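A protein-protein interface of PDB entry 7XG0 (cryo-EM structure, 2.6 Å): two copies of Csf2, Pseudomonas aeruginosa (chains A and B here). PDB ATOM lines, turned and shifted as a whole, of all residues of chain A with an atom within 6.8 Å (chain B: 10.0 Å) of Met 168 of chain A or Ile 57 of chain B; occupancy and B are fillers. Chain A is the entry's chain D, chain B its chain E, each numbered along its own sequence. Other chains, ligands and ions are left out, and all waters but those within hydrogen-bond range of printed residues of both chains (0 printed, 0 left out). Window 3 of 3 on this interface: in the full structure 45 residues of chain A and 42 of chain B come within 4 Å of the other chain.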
ATOM      1  N   ILE A 152     -13.862  -5.546   5.520  1.00  0.00           N
ATOM      2  CA  ILE A 152     -13.912  -4.234   6.154  1.00  0.00           C
ATOM      3  C   ILE A 152     -12.503  -3.663   6.131  1.00  0.00           C
ATOM      4  O   ILE A 152     -11.639  -4.043   6.929  1.00  0.00           O
ATOM      5  CB  ILE A 152     -14.494  -4.295   7.578  1.00  0.00           C
ATOM      6  CG1 ILE A 152     -15.934  -4.812   7.523  1.00  0.00           C
ATOM      7  CG2 ILE A 152     -14.454  -2.919   8.232  1.00  0.00           C
ATOM      8  CD1 ILE A 152     -16.641  -4.830   8.855  1.00  0.00           C
ATOM      9  N   HIS A 153     -12.272  -2.759   5.189  1.00  0.00           N
ATOM     10  CA  HIS A 153     -10.948  -2.304   4.812  1.00  0.00           C
ATOM     11  C   HIS A 153     -11.037  -0.821   4.485  1.00  0.00           C
ATOM     12  O   HIS A 153     -12.135  -0.283   4.312  1.00  0.00           O
ATOM     13  CB  HIS A 153     -10.435  -3.111   3.608  1.00  0.00           C
ATOM     14  CG  HIS A 153      -8.956  -3.041   3.398  1.00  0.00           C
ATOM     15  ND1 HIS A 153      -8.378  -2.283   2.403  1.00  0.00           N
ATOM     16  CD2 HIS A 153      -7.936  -3.657   4.042  1.00  0.00           C
ATOM     17  CE1 HIS A 153      -7.066  -2.425   2.450  1.00  0.00           C
ATOM     18  NE2 HIS A 153      -6.771  -3.252   3.437  1.00  0.00           N
ATOM     19  N   THR A 154      -9.877  -0.158   4.442  1.00  0.00           N
ATOM     20  CA  THR A 154      -9.841   1.241   4.027  1.00  0.00           C
ATOM     21  C   THR A 154     -10.283   1.405   2.581  1.00  0.00           C
ATOM     22  O   THR A 154     -10.996   2.363   2.254  1.00  0.00           O
ATOM     23  CB  THR A 154      -8.435   1.811   4.206  1.00  0.00           C
ATOM     24  OG1 THR A 154      -7.516   1.087   3.377  1.00  0.00           O
ATOM     25  CG2 THR A 154      -8.000   1.703   5.649  1.00  0.00           C
ATOM     26  N   ASN A 155      -9.922   0.440   1.725  1.00  0.00           N
ATOM     27  CA  ASN A 155     -10.249   0.474   0.303  1.00  0.00           C
ATOM     28  C   ASN A 155     -11.748   0.427   0.034  1.00  0.00           C
ATOM     29  O   ASN A 155     -12.172   0.777  -1.069  1.00  0.00           O
ATOM     30  CB  ASN A 155      -9.571  -0.694  -0.417  1.00  0.00           C
ATOM     31  CG  ASN A 155      -8.075  -0.505  -0.563  1.00  0.00           C
ATOM     32  OD1 ASN A 155      -7.505   0.465  -0.062  1.00  0.00           O
ATOM     33  ND2 ASN A 155      -7.427  -1.435  -1.257  1.00  0.00           N
ATOM     34  N   GLU A 157     -13.959   2.113   2.178  1.00  0.00           N
ATOM     35  CA  GLU A 157     -14.592   3.146   3.003  1.00  0.00           C
ATOM     36  C   GLU A 157     -15.645   3.950   2.248  1.00  0.00           C
ATOM     37  O   GLU A 157     -16.551   4.514   2.872  1.00  0.00           O
ATOM     38  CB  GLU A 157     -13.542   4.073   3.613  1.00  0.00           C
ATOM     39  CG  GLU A 157     -12.847   3.442   4.796  1.00  0.00           C
ATOM     40  CD  GLU A 157     -13.850   3.003   5.851  1.00  0.00           C
ATOM     41  OE1 GLU A 157     -14.683   3.837   6.266  1.00  0.00           O
ATOM     42  OE2 GLU A 157     -13.844   1.817   6.234  1.00  0.00           O
ATOM     43  N   LEU A 160     -18.358   1.135   2.610  1.00  0.00           N
ATOM     44  CA  LEU A 160     -18.879   0.826   3.939  1.00  0.00           C
ATOM     45  C   LEU A 160     -19.674   1.985   4.527  1.00  0.00           C
ATOM     46  O   LEU A 160     -20.727   1.773   5.140  1.00  0.00           O
ATOM     47  CB  LEU A 160     -17.731   0.452   4.875  1.00  0.00           C
ATOM     48  CG  LEU A 160     -17.025  -0.883   4.647  1.00  0.00           C
ATOM     49  CD1 LEU A 160     -15.593  -0.812   5.135  1.00  0.00           C
ATOM     50  CD2 LEU A 160     -17.767  -1.979   5.366  1.00  0.00           C
ATOM     51  N   TYR A 164     -17.974   1.873  10.772  1.00  0.00           N
ATOM     52  CA  TYR A 164     -17.106   0.720  10.570  1.00  0.00           C
ATOM     53  C   TYR A 164     -15.646   1.008  10.897  1.00  0.00           C
ATOM     54  O   TYR A 164     -14.756   0.387  10.307  1.00  0.00           O
ATOM     55  CB  TYR A 164     -17.239   0.215   9.134  1.00  0.00           C
ATOM     56  CG  TYR A 164     -18.449  -0.661   8.935  1.00  0.00           C
ATOM     57  CD1 TYR A 164     -18.579  -1.855   9.631  1.00  0.00           C
ATOM     58  CD2 TYR A 164     -19.471  -0.285   8.072  1.00  0.00           C
ATOM     59  CE1 TYR A 164     -19.684  -2.661   9.463  1.00  0.00           C
ATOM     60  CE2 TYR A 164     -20.584  -1.086   7.897  1.00  0.00           C
ATOM     61  CZ  TYR A 164     -20.681  -2.272   8.597  1.00  0.00           C
ATOM     62  OH  TYR A 164     -21.781  -3.073   8.432  1.00  0.00           O
ATOM     63  N   GLU A 165     -15.376   1.933  11.820  1.00  0.00           N
ATOM     64  CA  GLU A 165     -13.994   2.235  12.178  1.00  0.00           C
ATOM     65  C   GLU A 165     -13.445   1.224  13.181  1.00  0.00           C
ATOM     66  O   GLU A 165     -12.229   1.142  13.388  1.00  0.00           O
ATOM     67  CB  GLU A 165     -13.889   3.658  12.734  1.00  0.00           C
ATOM     68  CG  GLU A 165     -13.909   4.765  11.679  1.00  0.00           C
ATOM     69  CD  GLU A 165     -15.289   5.019  11.100  1.00  0.00           C
ATOM     70  OE1 GLU A 165     -16.289   4.690  11.772  1.00  0.00           O
ATOM     71  OE2 GLU A 165     -15.374   5.547   9.971  1.00  0.00           O
ATOM     72  N   ASN A 166     -14.325   0.450  13.813  1.00  0.00           N
ATOM     73  CA  ASN A 166     -13.891  -0.540  14.790  1.00  0.00           C
ATOM     74  C   ASN A 166     -13.389  -1.796  14.088  1.00  0.00           C
ATOM     75  O   ASN A 166     -13.951  -2.219  13.072  1.00  0.00           O
ATOM     76  CB  ASN A 166     -15.041  -0.884  15.737  1.00  0.00           C
ATOM     77  CG  ASN A 166     -16.347  -1.119  15.003  1.00  0.00           C
ATOM     78  OD1 ASN A 166     -16.861  -0.227  14.328  1.00  0.00           O
ATOM     79  ND2 ASN A 166     -16.894  -2.321  15.138  1.00  0.00           N
ATOM     80  N   GLU A 167     -12.332  -2.393  14.660  1.00  0.00           N
ATOM     81  CA  GLU A 167     -11.609  -3.546  14.096  1.00  0.00           C
ATOM     82  C   GLU A 167     -11.127  -3.252  12.673  1.00  0.00           C
ATOM     83  O   GLU A 167     -11.373  -4.012  11.735  1.00  0.00           O
ATOM     84  CB  GLU A 167     -12.455  -4.828  14.149  1.00  0.00           C
ATOM     85  CG  GLU A 167     -12.711  -5.358  15.564  1.00  0.00           C
ATOM     86  CD  GLU A 167     -13.138  -6.819  15.586  1.00  0.00           C
ATOM     87  OE1 GLU A 167     -13.482  -7.358  14.514  1.00  0.00           O
ATOM     88  OE2 GLU A 167     -13.146  -7.426  16.679  1.00  0.00           O
ATOM     89  N   MET A 168     -10.434  -2.125  12.521  1.00  0.00           N
ATOM     90  CA  MET A 168     -10.060  -1.601  11.214  1.00  0.00           C
ATOM     91  C   MET A 168      -8.906  -2.384  10.592  1.00  0.00           C
ATOM     92  O   MET A 168      -8.004  -2.859  11.283  1.00  0.00           O
ATOM     93  CB  MET A 168      -9.668  -0.129  11.341  1.00  0.00           C
ATOM     94  CG  MET A 168      -9.890   0.675  10.085  1.00  0.00           C
ATOM     95  SD  MET A 168     -11.271   0.030   9.132  1.00  0.00           S
ATOM     96  CE  MET A 168     -11.050   0.950   7.627  1.00  0.00           C
ATOM     97  N   MET A 169      -8.932  -2.489   9.261  1.00  0.00           N
ATOM     98  CA  MET A 169      -7.887  -3.141   8.478  1.00  0.00           C
ATOM     99  C   MET A 169      -7.298  -2.188   7.446  1.00  0.00           C
ATOM    100  O   MET A 169      -8.035  -1.473   6.759  1.00  0.00           O
ATOM    101  CB  MET A 169      -8.420  -4.389   7.772  1.00  0.00           C
ATOM    102  CG  MET A 169      -7.320  -5.231   7.158  1.00  0.00           C
ATOM    103  SD  MET A 169      -6.767  -6.659   8.073  1.00  0.00           S
ATOM    104  CE  MET A 169      -5.040  -6.615   7.667  1.00  0.00           C
ATOM    105  N   SER A 170      -5.968  -2.195   7.335  1.00  0.00           N
ATOM    106  CA  SER A 170      -5.237  -1.468   6.308  1.00  0.00           C
ATOM    107  C   SER A 170      -4.296  -2.430   5.594  1.00  0.00           C
ATOM    108  O   SER A 170      -4.047  -3.545   6.059  1.00  0.00           O
ATOM    109  CB  SER A 170      -4.434  -0.301   6.903  1.00  0.00           C
ATOM    110  OG  SER A 170      -5.266   0.793   7.245  1.00  0.00           O
ATOM    111  N   GLY A 255      -8.913 -14.310   9.296  1.00  0.00           N
ATOM    112  CA  GLY A 255      -9.067 -13.374  10.388  1.00  0.00           C
ATOM    113  C   GLY A 255      -9.745 -12.073  10.030  1.00  0.00           C
ATOM    114  O   GLY A 255      -9.978 -11.252  10.926  1.00  0.00           O
ATOM    115  N   LEU A 256     -10.068 -11.855   8.758  1.00  0.00           N
ATOM    116  CA  LEU A 256     -10.697 -10.610   8.351  1.00  0.00           C
ATOM    117  C   LEU A 256     -12.151 -10.564   8.800  1.00  0.00           C
ATOM    118  O   LEU A 256     -12.846 -11.580   8.858  1.00  0.00           O
ATOM    119  CB  LEU A 256     -10.649 -10.435   6.833  1.00  0.00           C
ATOM    120  CG  LEU A 256      -9.324 -10.386   6.078  1.00  0.00           C
ATOM    121  CD1 LEU A 256      -9.535  -9.655   4.770  1.00  0.00           C
ATOM    122  CD2 LEU A 256      -8.238  -9.727   6.887  1.00  0.00           C
ATOM    123  N   LYS A 257     -12.614  -9.360   9.108  1.00  0.00           N
ATOM    124  CA  LYS A 257     -14.025  -9.111   9.350  1.00  0.00           C
ATOM    125  C   LYS A 257     -14.638  -8.590   8.058  1.00  0.00           C
ATOM    126  O   LYS A 257     -14.143  -7.618   7.479  1.00  0.00           O
ATOM    127  CB  LYS A 257     -14.229  -8.115  10.491  1.00  0.00           C
ATOM    128  CG  LYS A 257     -15.685  -7.819  10.796  1.00  0.00           C
ATOM    129  CD  LYS A 257     -15.918  -7.641  12.286  1.00  0.00           C
ATOM    130  CE  LYS A 257     -17.158  -6.805  12.556  1.00  0.00           C
ATOM    131  NZ  LYS A 257     -16.882  -5.347  12.425  1.00  0.00           N
ATOM    132  N   VAL B  48      -2.062 -13.572   8.902  1.00  0.00           N
ATOM    133  CA  VAL B  48      -3.319 -13.621   9.633  1.00  0.00           C
ATOM    134  C   VAL B  48      -3.601 -12.241  10.205  1.00  0.00           C
ATOM    135  O   VAL B  48      -2.686 -11.490  10.553  1.00  0.00           O
ATOM    136  CB  VAL B  48      -3.309 -14.689  10.751  1.00  0.00           C
ATOM    137  CG1 VAL B  48      -3.366 -16.086  10.163  1.00  0.00           C
ATOM    138  CG2 VAL B  48      -2.059 -14.551  11.600  1.00  0.00           C
ATOM    139  N   ALA B  49      -4.880 -11.896  10.270  1.00  0.00           N
ATOM    140  CA  ALA B  49      -5.285 -10.652  10.905  1.00  0.00           C
ATOM    141  C   ALA B  49      -5.248 -10.825  12.418  1.00  0.00           C
ATOM    142  O   ALA B  49      -5.774 -11.808  12.949  1.00  0.00           O
ATOM    143  CB  ALA B  49      -6.680 -10.246  10.438  1.00  0.00           C
ATOM    144  N   ALA B  50      -4.613  -9.880  13.107  1.00  0.00           N
ATOM    145  CA  ALA B  50      -4.448  -9.966  14.551  1.00  0.00           C
ATOM    146  C   ALA B  50      -4.491  -8.576  15.161  1.00  0.00           C
ATOM    147  O   ALA B  50      -4.033  -7.603  14.560  1.00  0.00           O
ATOM    148  CB  ALA B  50      -3.130 -10.644  14.932  1.00  0.00           C
ATOM    149  N   ASP B  51      -5.035  -8.498  16.372  1.00  0.00           N
ATOM    150  CA  ASP B  51      -5.100  -7.244  17.110  1.00  0.00           C
ATOM    151  C   ASP B  51      -3.729  -6.913  17.692  1.00  0.00           C
ATOM    152  O   ASP B  51      -3.257  -7.592  18.609  1.00  0.00           O
ATOM    153  CB  ASP B  51      -6.173  -7.343  18.196  1.00  0.00           C
ATOM    154  CG  ASP B  51      -6.097  -6.225  19.200  1.00  0.00           C
ATOM    155  OD1 ASP B  51      -6.703  -5.167  18.946  1.00  0.00           O
ATOM    156  OD2 ASP B  51      -5.436  -6.411  20.245  1.00  0.00           O
ATOM    157  N   VAL B  52      -3.083  -5.874  17.164  1.00  0.00           N
ATOM    158  CA  VAL B  52      -1.683  -5.618  17.496  1.00  0.00           C
ATOM    159  C   VAL B  52      -1.535  -4.376  18.372  1.00  0.00           C
ATOM    160  O   VAL B  52      -0.611  -4.283  19.188  1.00  0.00           O
ATOM    161  CB  VAL B  52      -0.833  -5.532  16.211  1.00  0.00           C
ATOM    162  CG1 VAL B  52      -0.899  -6.846  15.467  1.00  0.00           C
ATOM    163  CG2 VAL B  52      -1.324  -4.423  15.293  1.00  0.00           C
ATOM    164  N   GLY B  53      -2.433  -3.404  18.220  1.00  0.00           N
ATOM    165  CA  GLY B  53      -2.324  -2.168  18.972  1.00  0.00           C
ATOM    166  C   GLY B  53      -3.450  -1.984  19.966  1.00  0.00           C
ATOM    167  O   GLY B  53      -3.757  -0.854  20.360  1.00  0.00           O
ATOM    168  N   ASP B  54      -4.112  -3.102  20.300  1.00  0.00           N
ATOM    169  CA  ASP B  54      -5.226  -3.264  21.241  1.00  0.00           C
ATOM    170  C   ASP B  54      -6.530  -2.618  20.765  1.00  0.00           C
ATOM    171  O   ASP B  54      -7.577  -2.801  21.396  1.00  0.00           O
ATOM    172  CB  ASP B  54      -4.856  -2.745  22.639  1.00  0.00           C
ATOM    173  CG  ASP B  54      -5.428  -3.604  23.748  1.00  0.00           C
ATOM    174  OD1 ASP B  54      -5.973  -4.686  23.443  1.00  0.00           O
ATOM    175  OD2 ASP B  54      -5.330  -3.200  24.926  1.00  0.00           O
ATOM    176  N   GLY B  55      -6.487  -1.874  19.662  1.00  0.00           N
ATOM    177  CA  GLY B  55      -7.673  -1.459  18.942  1.00  0.00           C
ATOM    178  C   GLY B  55      -7.572  -1.786  17.466  1.00  0.00           C
ATOM    179  O   GLY B  55      -8.585  -1.946  16.780  1.00  0.00           O
ATOM    180  N   VAL B  56      -6.339  -1.893  16.971  1.00  0.00           N
ATOM    181  CA  VAL B  56      -6.052  -1.953  15.542  1.00  0.00           C
ATOM    182  C   VAL B  56      -5.604  -3.361  15.182  1.00  0.00           C
ATOM    183  O   VAL B  56      -4.667  -3.902  15.784  1.00  0.00           O
ATOM    184  CB  VAL B  56      -4.982  -0.908  15.162  1.00  0.00           C
ATOM    185  CG1 VAL B  56      -4.306  -1.247  13.830  1.00  0.00           C
ATOM    186  CG2 VAL B  56      -5.589   0.484  15.124  1.00  0.00           C
ATOM    187  N   ILE B  57      -6.263  -3.956  14.191  1.00  0.00           N
ATOM    188  CA  ILE B  57      -5.931  -5.291  13.719  1.00  0.00           C
ATOM    189  C   ILE B  57      -5.204  -5.158  12.382  1.00  0.00           C
ATOM    190  O   ILE B  57      -5.531  -4.295  11.559  1.00  0.00           O
ATOM    191  CB  ILE B  57      -7.193  -6.191  13.688  1.00  0.00           C
ATOM    192  CG1 ILE B  57      -8.140  -5.931  12.516  1.00  0.00           C
ATOM    193  CG2 ILE B  57      -7.993  -6.052  14.977  1.00  0.00           C
ATOM    194  CD1 ILE B  57      -7.999  -6.900  11.400  1.00  0.00           C
ATOM    195  N   LYS B  58      -4.166  -5.976  12.203  1.00  0.00           N
ATOM    196  CA  LYS B  58      -3.217  -5.840  11.106  1.00  0.00           C
ATOM    197  C   LYS B  58      -2.790  -7.237  10.663  1.00  0.00           C
ATOM    198  O   LYS B  58      -2.924  -8.211  11.410  1.00  0.00           O
ATOM    199  CB  LYS B  58      -2.029  -4.953  11.567  1.00  0.00           C
ATOM    200  CG  LYS B  58      -0.829  -4.706  10.619  1.00  0.00           C
ATOM    201  CD  LYS B  58       0.298  -3.852  11.243  1.00  0.00           C
ATOM    202  CE  LYS B  58      -0.132  -2.718  12.210  1.00  0.00           C
ATOM    203  NZ  LYS B  58      -1.236  -1.809  11.760  1.00  0.00           N
ATOM    204  N   SER B  59      -2.306  -7.329   9.422  1.00  0.00           N
ATOM    205  CA  SER B  59      -1.869  -8.586   8.817  1.00  0.00           C
ATOM    206  C   SER B  59      -0.462  -8.877   9.311  1.00  0.00           C
ATOM    207  O   SER B  59       0.478  -8.136   9.017  1.00  0.00           O
ATOM    208  CB  SER B  59      -1.906  -8.490   7.297  1.00  0.00           C
ATOM    209  OG  SER B  59      -1.503  -9.703   6.691  1.00  0.00           O
ATOM    210  N   VAL B  60      -0.314  -9.950  10.079  1.00  0.00           N
ATOM    211  CA  VAL B  60       0.960 -10.332  10.685  1.00  0.00           C
ATOM    212  C   VAL B  60       1.350 -11.731  10.212  1.00  0.00           C
ATOM    213  O   VAL B  60       0.472 -12.520   9.829  1.00  0.00           O
ATOM    214  CB  VAL B  60       0.882 -10.249  12.221  1.00  0.00           C
ATOM    215  CG1 VAL B  60       0.558  -8.837  12.663  1.00  0.00           C
ATOM    216  CG2 VAL B  60      -0.174 -11.198  12.748  1.00  0.00           C
ATOM    217  N   THR B 154      -0.945 -15.717  19.788  1.00  0.00           N
ATOM    218  CA  THR B 154      -1.738 -14.494  19.848  1.00  0.00           C
ATOM    219  C   THR B 154      -1.907 -13.844  18.481  1.00  0.00           C
ATOM    220  O   THR B 154      -2.799 -13.005  18.312  1.00  0.00           O
ATOM    221  CB  THR B 154      -1.109 -13.501  20.827  1.00  0.00           C
ATOM    222  OG1 THR B 154       0.284 -13.349  20.528  1.00  0.00           O
ATOM    223  CG2 THR B 154      -1.267 -13.999  22.255  1.00  0.00           C
ATOM    224  N   ASN B 155      -1.068 -14.203  17.507  1.00  0.00           N
ATOM    225  CA  ASN B 155      -1.297 -13.781  16.131  1.00  0.00           C
ATOM    226  C   ASN B 155      -2.519 -14.477  15.541  1.00  0.00           C
ATOM    227  O   ASN B 155      -3.187 -13.931  14.657  1.00  0.00           O
ATOM    228  CB  ASN B 155      -0.055 -14.061  15.286  1.00  0.00           C
ATOM    229  CG  ASN B 155       1.054 -13.058  15.532  1.00  0.00           C
ATOM    230  OD1 ASN B 155       0.965 -12.225  16.434  1.00  0.00           O
ATOM    231  ND2 ASN B 155       2.111 -13.136  14.731  1.00  0.00           N
ATOM    232  N   GLU B 157      -5.244 -15.158  17.289  1.00  0.00           N
ATOM    233  CA  GLU B 157      -6.315 -14.984  18.269  1.00  0.00           C
ATOM    234  C   GLU B 157      -7.662 -14.724  17.598  1.00  0.00           C
ATOM    235  O   GLU B 157      -8.717 -14.961  18.197  1.00  0.00           O
ATOM    236  CB  GLU B 157      -5.951 -13.848  19.232  1.00  0.00           C
ATOM    237  CG  GLU B 157      -6.474 -12.424  18.912  1.00  0.00           C
ATOM    238  CD  GLU B 157      -5.876 -11.744  17.663  1.00  0.00           C
ATOM    239  OE1 GLU B 157      -5.667 -12.365  16.599  1.00  0.00           O
ATOM    240  OE2 GLU B 157      -5.597 -10.534  17.763  1.00  0.00           O
ATOM    241  N   ARG B 158      -7.648 -14.240  16.353  1.00  0.00           N
ATOM    242  CA  ARG B 158      -8.888 -14.160  15.587  1.00  0.00           C
ATOM    243  C   ARG B 158      -9.156 -15.463  14.844  1.00  0.00           C
ATOM    244  O   ARG B 158     -10.239 -15.652  14.281  1.00  0.00           O
ATOM    245  CB  ARG B 158      -8.834 -12.982  14.615  1.00  0.00           C
ATOM    246  CG  ARG B 158      -8.814 -11.621  15.296  1.00  0.00           C
ATOM    247  CD  ARG B 158      -8.498 -10.509  14.310  1.00  0.00           C
ATOM    248  NE  ARG B 158      -9.585 -10.284  13.364  1.00  0.00           N
ATOM    249  CZ  ARG B 158     -10.581  -9.432  13.558  1.00  0.00           C
ATOM    250  NH1 ARG B 158     -10.660  -8.699  14.656  1.00  0.00           N
ATOM    251  NH2 ARG B 158     -11.522  -9.312  12.626  1.00  0.00           N
ATOM    252  N   ILE B 159      -8.181 -16.376  14.833  1.00  0.00           N
ATOM    253  CA  ILE B 159      -8.357 -17.638  14.121  1.00  0.00           C
ATOM    254  C   ILE B 159      -8.975 -18.686  15.038  1.00  0.00           C
ATOM    255  O   ILE B 159      -9.915 -19.392  14.650  1.00  0.00           O
ATOM    256  CB  ILE B 159      -7.016 -18.118  13.531  1.00  0.00           C
ATOM    257  CG1 ILE B 159      -6.383 -17.044  12.639  1.00  0.00           C
ATOM    258  CG2 ILE B 159      -7.199 -19.407  12.745  1.00  0.00           C
ATOM    259  CD1 ILE B 159      -7.316 -16.449  11.607  1.00  0.00           C
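Positions printed for both chains: 154, 155 and 157.
Printed residues of chain A that touch a printed residue of chain B: Glu 167, Met 168, Met 169, Gly 255, Leu 256 and Lys 257.
Hydrophobic or aromatic side chains of chain A that line the printed part of chain B: Met 169 and Leu 256.
Of the 18 printed residues of chain B, 6 touch a printed residue of chain A.
Hydrophobic or aromatic side chains of chain B that line the printed part of chain A: Ala 49, Ile 57 and Ile 159.
The backbone carbonyl oxygen (O) of Ala 50 of chain B is in hydrogen-bond range of the backbone NH (N) of Lys 58 of chain B (2.9 Å).
N of Thr 154 of chain A is in hydrogen-bond range of O of Met 169 of chain A, at 3.2 Å.
The backbone NH of Ile 152 of chain A is in hydrogen-bond range of the backbone carbonyl oxygen of Lys 257 of chain A.
Printed residues of chain B within 4 Å of Met 168 of chain A: Ile 57 (2.9 Å).
Of chain A, only Glu 167 (3.8 Å), Met 168 (2.9 Å) and Met 169 (3.6 Å) come within 4 Å of Ile 57 of chain B.
Met 169 of chain A touches three residues of chain B.
Printed residues of chain B within 4 Å of Leu 256 of chain A: Ala 49.
Printed residues of chain A within 4 Å of Ser 59 of chain B: Met 169.
Printed residues of chain A within 4 Å of Arg 158 of chain B: Glu 167 (3.1 Å), Gly 255 (2.7 Å) and Lys 257 (3.6 Å).
His 153 of chain A touches none of the printed residues of chain B.
The nearest residue of chain B that does not touch Met 168 of chain A is Val 56 of chain B (4.6 Å).
Among the printed residues, pairs that only touch across the chains: Met 169 of chain A with Ser 59 of chain B (3.3 Å), Gly 255 of chain A with Ala 49 of chain B (3.5 Å), Gly 255 of chain A with Ile 159 of chain B (3.5 Å), Met 169 of chain A with Ile 57 of chain B (3.6 Å), Lys 257 of chain A with Arg 158 of chain B (3.6 Å), Met 169 of chain A with Lys 58 of chain B (3.8 Å), Glu 167 of chain A with Ile 57 of chain B (3.8 Å) and Leu 256 of chain A with Ala 49 of chain B (3.9 Å).
The backbone carbonyl oxygen (O) of Gly 255 of chain A lies within hydrogen-bond range of the guanidinium group (NE) of Arg 158 of chain B (2.7 Å).
The side-chain carboxylate (OE1) of Glu 167 of chain A lies within salt-bridge range of the guanidinium group (NH1) of Arg 158 of chain B, 3.1 Å away.
O of Met 168 of chain A lies close to O of Ile 57 of chain B (2.9 Å).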
